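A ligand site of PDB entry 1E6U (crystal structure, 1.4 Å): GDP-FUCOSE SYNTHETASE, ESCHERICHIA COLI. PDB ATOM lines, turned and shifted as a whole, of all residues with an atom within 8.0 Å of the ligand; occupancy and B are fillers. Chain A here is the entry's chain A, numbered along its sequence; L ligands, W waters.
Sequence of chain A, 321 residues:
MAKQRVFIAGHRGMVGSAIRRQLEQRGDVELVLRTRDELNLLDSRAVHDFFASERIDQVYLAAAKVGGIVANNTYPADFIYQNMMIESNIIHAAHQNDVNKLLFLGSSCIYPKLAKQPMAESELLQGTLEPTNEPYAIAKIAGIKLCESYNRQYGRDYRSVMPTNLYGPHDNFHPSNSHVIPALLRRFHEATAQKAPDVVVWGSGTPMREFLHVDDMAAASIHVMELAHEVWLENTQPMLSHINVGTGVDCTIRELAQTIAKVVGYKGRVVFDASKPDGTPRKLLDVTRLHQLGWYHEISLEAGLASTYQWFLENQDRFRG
N of Gly 68 lies within hydrogen-bond range of O1 of the ligand (3.1 Å). N of Val 70 is in hydrogen-bond range of O3 of the ligand (2.9 Å). The backbone NH (N) of Ala 71 is in hydrogen-bond range of an oxygen (O2) of the ligand (3.1 Å). OG of Ser 178 lies within hydrogen-bond range of O4 of the ligand. N of Ser 178 lies within hydrogen-bond range of O4 of the ligand. The backbone NH (N) of Ile 69 is in hydrogen-bond range of an oxygen (O3) of the ligand (3.2 Å).
ND2 of Asn 177 lies within hydrogen-bond range of O of Asn 172 (2.9 Å). The backbone NH (N) of Ile 69 is in hydrogen-bond range of the side-chain hydroxyl (OG) of Ser 178 (3.0 Å). O of Ile 69 lies within hydrogen-bond range of ND2 of Asn 73 (3.0 Å). O of Gly 68 is in hydrogen-bond range of ND2 of Asn 72, at 3.0 Å. The backbone carbonyl oxygen (O) of Val 70 sits at hydrogen-bond distance from the side-chain hydroxyl (OG1) of Thr 74. ND2 of Asn 72 is in hydrogen-bond range of O of Gly 67, 3.0 Å away. N of His 179 sits at hydrogen-bond distance from OD1 of Asn 177 (2.9 Å).
Gly 67 touches the ligand. OD1 of Asn 177 touches O4 of the ligand, at 3.7 Å. The nearest printed residue that does not touch the ligand is Ser 176 (4.2 Å).
Water W3 lies within hydrogen-bond range of OD1 of Asn 177 (2.8 Å), O4 of the ligand (2.9 Å), ND1 of His 179 (3.2 Å) and N of Gly 68 (3.2 Å).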
ATOM      1  N   LYS A  65     -17.327   8.503 -28.953  1.00  0.00           N
ATOM      2  CA  LYS A  65     -16.941   9.806 -28.434  1.00  0.00           C
ATOM      3  C   LYS A  65     -15.452   9.698 -28.094  1.00  0.00           C
ATOM      4  O   LYS A  65     -15.080   8.925 -27.199  1.00  0.00           O
ATOM      5  CB  LYS A  65     -17.770  10.232 -27.190  1.00  0.00           C
ATOM      6  CG  LYS A  65     -17.340  11.663 -26.808  1.00  0.00           C
ATOM      7  CD  LYS A  65     -17.994  12.490 -25.798  1.00  0.00           C
ATOM      8  CE  LYS A  65     -17.279  13.808 -25.657  1.00  0.00           C
ATOM      9  NZ  LYS A  65     -17.568  14.785 -26.749  1.00  0.00           N
ATOM     10  N   VAL A  66     -14.647  10.448 -28.836  1.00  0.00           N
ATOM     11  CA  VAL A  66     -13.177  10.384 -28.732  1.00  0.00           C
ATOM     12  C   VAL A  66     -12.624  11.780 -28.527  1.00  0.00           C
ATOM     13  O   VAL A  66     -13.200  12.735 -29.082  1.00  0.00           O
ATOM     14  CB  VAL A  66     -12.644   9.801 -30.065  1.00  0.00           C
ATOM     15  CG1 VAL A  66     -11.153   9.575 -30.076  1.00  0.00           C
ATOM     16  CG2 VAL A  66     -13.316   8.465 -30.317  1.00  0.00           C
ATOM     17  N   GLY A  67     -11.525  11.867 -27.775  1.00  0.00           N
ATOM     18  CA  GLY A  67     -10.882  13.175 -27.581  1.00  0.00           C
ATOM     19  C   GLY A  67      -9.489  12.949 -27.005  1.00  0.00           C
ATOM     20  O   GLY A  67      -9.031  11.840 -26.759  1.00  0.00           O
ATOM     21  N   GLY A  68      -8.861  14.083 -26.696  1.00  0.00           N
ATOM     22  CA  GLY A  68      -7.541  14.111 -26.101  1.00  0.00           C
ATOM     23  C   GLY A  68      -7.547  14.248 -24.610  1.00  0.00           C
ATOM     24  O   GLY A  68      -8.539  13.937 -23.925  1.00  0.00           O
ATOM     25  N   ILE A  69      -6.403  14.650 -24.042  1.00  0.00           N
ATOM     26  CA  ILE A  69      -6.259  14.661 -22.596  1.00  0.00           C
ATOM     27  C   ILE A  69      -7.210  15.654 -21.931  1.00  0.00           C
ATOM     28  O   ILE A  69      -7.765  15.276 -20.888  1.00  0.00           O
ATOM     29  CB  ILE A  69      -4.810  14.905 -22.217  1.00  0.00           C
ATOM     30  CG1 ILE A  69      -3.902  13.750 -22.671  1.00  0.00           C
ATOM     31  CG2 ILE A  69      -4.609  15.251 -20.759  1.00  0.00           C
ATOM     32  CD1 ILE A  69      -2.464  14.232 -22.586  1.00  0.00           C
ATOM     33  N   VAL A  70      -7.347  16.858 -22.447  1.00  0.00           N
ATOM     34  CA  VAL A  70      -8.239  17.817 -21.785  1.00  0.00           C
ATOM     35  C   VAL A  70      -9.652  17.296 -21.852  1.00  0.00           C
ATOM     36  O   VAL A  70     -10.368  17.296 -20.841  1.00  0.00           O
ATOM     37  CB  VAL A  70      -8.126  19.217 -22.392  1.00  0.00           C
ATOM     38  CG1 VAL A  70      -9.209  20.142 -21.811  1.00  0.00           C
ATOM     39  CG2 VAL A  70      -6.728  19.767 -22.141  1.00  0.00           C
ATOM     40  N   ALA A  71     -10.073  16.798 -23.022  1.00  0.00           N
ATOM     41  CA  ALA A  71     -11.462  16.355 -23.166  1.00  0.00           C
ATOM     42  C   ALA A  71     -11.764  15.192 -22.239  1.00  0.00           C
ATOM     43  O   ALA A  71     -12.797  15.205 -21.585  1.00  0.00           O
ATOM     44  CB  ALA A  71     -11.705  15.950 -24.624  1.00  0.00           C
ATOM     45  N   ASN A  72     -10.889  14.206 -22.180  1.00  0.00           N
ATOM     46  CA  ASN A  72     -11.148  13.037 -21.355  1.00  0.00           C
ATOM     47  C   ASN A  72     -11.218  13.410 -19.881  1.00  0.00           C
ATOM     48  O   ASN A  72     -11.957  12.733 -19.134  1.00  0.00           O
ATOM     49  CB  ASN A  72     -10.087  11.938 -21.573  1.00  0.00           C
ATOM     50  CG  ASN A  72     -10.464  11.057 -22.762  1.00  0.00           C
ATOM     51  OD1 ASN A  72     -11.156  10.045 -22.601  1.00  0.00           O
ATOM     52  ND2 ASN A  72     -10.071  11.390 -23.961  1.00  0.00           N
ATOM     53  N   ASN A  73     -10.404  14.334 -19.398  1.00  0.00           N
ATOM     54  CA  ASN A  73     -10.483  14.724 -17.997  1.00  0.00           C
ATOM     55  C   ASN A  73     -11.600  15.724 -17.698  1.00  0.00           C
ATOM     56  O   ASN A  73     -11.992  15.816 -16.530  1.00  0.00           O
ATOM     57  CB  ASN A  73      -9.163  15.405 -17.600  1.00  0.00           C
ATOM     58  CG  ASN A  73      -8.084  14.393 -17.298  1.00  0.00           C
ATOM     59  OD1 ASN A  73      -8.149  13.654 -16.316  1.00  0.00           O
ATOM     60  ND2 ASN A  73      -7.039  14.418 -18.055  1.00  0.00           N
ATOM     61  N   THR A  74     -12.070  16.432 -18.732  1.00  0.00           N
ATOM     62  CA  THR A  74     -13.085  17.444 -18.476  1.00  0.00           C
ATOM     63  C   THR A  74     -14.498  16.918 -18.574  1.00  0.00           C
ATOM     64  O   THR A  74     -15.404  17.411 -17.909  1.00  0.00           O
ATOM     65  CB  THR A  74     -12.848  18.578 -19.485  1.00  0.00           C
ATOM     66  OG1 THR A  74     -11.540  19.140 -19.225  1.00  0.00           O
ATOM     67  CG2 THR A  74     -13.840  19.710 -19.404  1.00  0.00           C
ATOM     68  N   TYR A  75     -14.719  15.927 -19.473  1.00  0.00           N
ATOM     69  CA  TYR A  75     -16.049  15.406 -19.729  1.00  0.00           C
ATOM     70  C   TYR A  75     -16.118  13.895 -19.460  1.00  0.00           C
ATOM     71  O   TYR A  75     -16.538  13.132 -20.334  1.00  0.00           O
ATOM     72  CB  TYR A  75     -16.489  15.689 -21.168  1.00  0.00           C
ATOM     73  CG  TYR A  75     -16.378  17.158 -21.564  1.00  0.00           C
ATOM     74  CD1 TYR A  75     -17.353  18.055 -21.146  1.00  0.00           C
ATOM     75  CD2 TYR A  75     -15.278  17.641 -22.265  1.00  0.00           C
ATOM     76  CE1 TYR A  75     -17.242  19.407 -21.447  1.00  0.00           C
ATOM     77  CE2 TYR A  75     -15.176  18.995 -22.570  1.00  0.00           C
ATOM     78  CZ  TYR A  75     -16.196  19.849 -22.211  1.00  0.00           C
ATOM     79  OH  TYR A  75     -16.104  21.198 -22.496  1.00  0.00           O
ATOM     80  N   PHE A  79     -17.760  10.685 -21.811  1.00  0.00           N
ATOM     81  CA  PHE A  79     -16.950   9.660 -22.464  1.00  0.00           C
ATOM     82  C   PHE A  79     -17.408   8.265 -22.080  1.00  0.00           C
ATOM     83  O   PHE A  79     -17.450   7.384 -22.942  1.00  0.00           O
ATOM     84  CB  PHE A  79     -15.460   9.867 -22.181  1.00  0.00           C
ATOM     85  CG  PHE A  79     -14.821  10.848 -23.128  1.00  0.00           C
ATOM     86  CD1 PHE A  79     -14.277  10.440 -24.305  1.00  0.00           C
ATOM     87  CD2 PHE A  79     -14.793  12.183 -22.833  1.00  0.00           C
ATOM     88  CE1 PHE A  79     -13.773  11.336 -25.213  1.00  0.00           C
ATOM     89  CE2 PHE A  79     -14.305  13.127 -23.748  1.00  0.00           C
ATOM     90  CZ  PHE A  79     -13.762  12.667 -24.912  1.00  0.00           C
ATOM     91  N   THR A 132      -6.373   9.589 -16.731  1.00  0.00           N
ATOM     92  CA  THR A 132      -6.956  10.483 -17.732  1.00  0.00           C
ATOM     93  C   THR A 132      -7.935   9.737 -18.591  1.00  0.00           C
ATOM     94  O   THR A 132      -8.965  10.295 -18.947  1.00  0.00           O
ATOM     95  CB  THR A 132      -5.835  11.049 -18.577  1.00  0.00           C
ATOM     96  OG1 THR A 132      -5.202  12.074 -17.813  1.00  0.00           O
ATOM     97  CG2 THR A 132      -6.335  11.627 -19.894  1.00  0.00           C
ATOM     98  N   ASN A 172      -7.408  15.851 -36.357  1.00  0.00           N
ATOM     99  CA  ASN A 172      -7.565  17.240 -35.912  1.00  0.00           C
ATOM    100  C   ASN A 172      -6.229  17.969 -35.882  1.00  0.00           C
ATOM    101  O   ASN A 172      -5.473  17.824 -34.909  1.00  0.00           O
ATOM    102  CB  ASN A 172      -8.193  17.245 -34.501  1.00  0.00           C
ATOM    103  CG  ASN A 172      -8.280  18.634 -33.932  1.00  0.00           C
ATOM    104  OD1 ASN A 172      -8.396  18.833 -32.715  1.00  0.00           O
ATOM    105  ND2 ASN A 172      -8.177  19.681 -34.749  1.00  0.00           N
ATOM    106  N   HIS A 174      -4.650  20.814 -35.086  1.00  0.00           N
ATOM    107  CA  HIS A 174      -4.707  22.048 -34.282  1.00  0.00           C
ATOM    108  C   HIS A 174      -3.482  21.975 -33.391  1.00  0.00           C
ATOM    109  O   HIS A 174      -3.181  20.878 -32.909  1.00  0.00           O
ATOM    110  CB  HIS A 174      -6.025  22.085 -33.507  1.00  0.00           C
ATOM    111  CG  HIS A 174      -6.121  23.337 -32.678  1.00  0.00           C
ATOM    112  ND1 HIS A 174      -5.307  23.570 -31.585  1.00  0.00           N
ATOM    113  CD2 HIS A 174      -6.920  24.429 -32.780  1.00  0.00           C
ATOM    114  CE1 HIS A 174      -5.578  24.763 -31.077  1.00  0.00           C
ATOM    115  NE2 HIS A 174      -6.570  25.298 -31.772  1.00  0.00           N
ATOM    116  N   SER A 176      -2.877  22.742 -30.466  1.00  0.00           N
ATOM    117  CA  SER A 176      -3.062  22.387 -29.056  1.00  0.00           C
ATOM    118  C   SER A 176      -3.603  20.989 -28.875  1.00  0.00           C
ATOM    119  O   SER A 176      -3.788  20.564 -27.699  1.00  0.00           O
ATOM    120  CB  SER A 176      -4.053  23.380 -28.427  1.00  0.00           C
ATOM    121  OG  SER A 176      -3.292  24.637 -28.385  1.00  0.00           O
ATOM    122  N   ASN A 177      -3.746  20.225 -29.966  1.00  0.00           N
ATOM    123  CA  ASN A 177      -4.133  18.815 -29.858  1.00  0.00           C
ATOM    124  C   ASN A 177      -3.155  18.106 -28.948  1.00  0.00           C
ATOM    125  O   ASN A 177      -1.934  18.242 -29.115  1.00  0.00           O
ATOM    126  CB  ASN A 177      -4.264  18.163 -31.235  1.00  0.00           C
ATOM    127  CG  ASN A 177      -4.933  16.819 -31.266  1.00  0.00           C
ATOM    128  OD1 ASN A 177      -5.037  16.109 -30.251  1.00  0.00           O
ATOM    129  ND2 ASN A 177      -5.366  16.327 -32.431  1.00  0.00           N
ATOM    130  N   SER A 178      -3.656  17.287 -28.015  1.00  0.00           N
ATOM    131  CA  SER A 178      -2.728  16.523 -27.186  1.00  0.00           C
ATOM    132  C   SER A 178      -2.117  15.354 -27.961  1.00  0.00           C
ATOM    133  O   SER A 178      -1.105  14.805 -27.505  1.00  0.00           O
ATOM    134  CB  SER A 178      -3.398  16.101 -25.889  1.00  0.00           C
ATOM    135  OG  SER A 178      -4.473  15.241 -26.197  1.00  0.00           O
ATOM    136  N   HIS A 179      -2.683  14.919 -29.068  1.00  0.00           N
ATOM    137  CA  HIS A 179      -2.096  13.881 -29.896  1.00  0.00           C
ATOM    138  C   HIS A 179      -0.894  14.423 -30.684  1.00  0.00           C
ATOM    139  O   HIS A 179      -1.025  15.384 -31.420  1.00  0.00           O
ATOM    140  CB  HIS A 179      -3.139  13.269 -30.823  1.00  0.00           C
ATOM    141  CG  HIS A 179      -4.255  12.629 -30.044  1.00  0.00           C
ATOM    142  ND1 HIS A 179      -5.542  13.040 -30.181  1.00  0.00           N
ATOM    143  CD2 HIS A 179      -4.258  11.692 -29.089  1.00  0.00           C
ATOM    144  CE1 HIS A 179      -6.328  12.332 -29.399  1.00  0.00           C
ATOM    145  NE2 HIS A 179      -5.585  11.501 -28.718  1.00  0.00           N
HETATM  146  C1  LIG L   1      -9.509  17.675 -26.709  1.00  0.00           C
HETATM  147  O1  LIG L   1     -10.002  16.838 -27.525  1.00  0.00           O
HETATM  148  C2  LIG L   1     -10.032  18.756 -26.306  1.00  0.00           C
HETATM  149  O2  LIG L   1      -8.525  17.015 -25.646  1.00  0.00           O
HETATM  150  P1  LIG L   1      -7.321  17.815 -25.963  1.00  0.00           P
HETATM  151  O3  LIG L   1      -6.253  17.647 -25.016  1.00  0.00           O
HETATM  152  O4  LIG L   1      -6.831  17.187 -27.180  1.00  0.00           O
HETATM  153  O5  LIG L   1      -7.557  19.312 -26.403  1.00  0.00           O
HETATM  154  O   HOH W   1     -11.963  19.624 -24.169  1.00  0.00           O
HETATM  155  O   HOH W   2      -7.717  19.508 -29.325  1.00  0.00           O
HETATM  156  O   HOH W   3      -7.559  15.384 -29.364  1.00  0.00           O
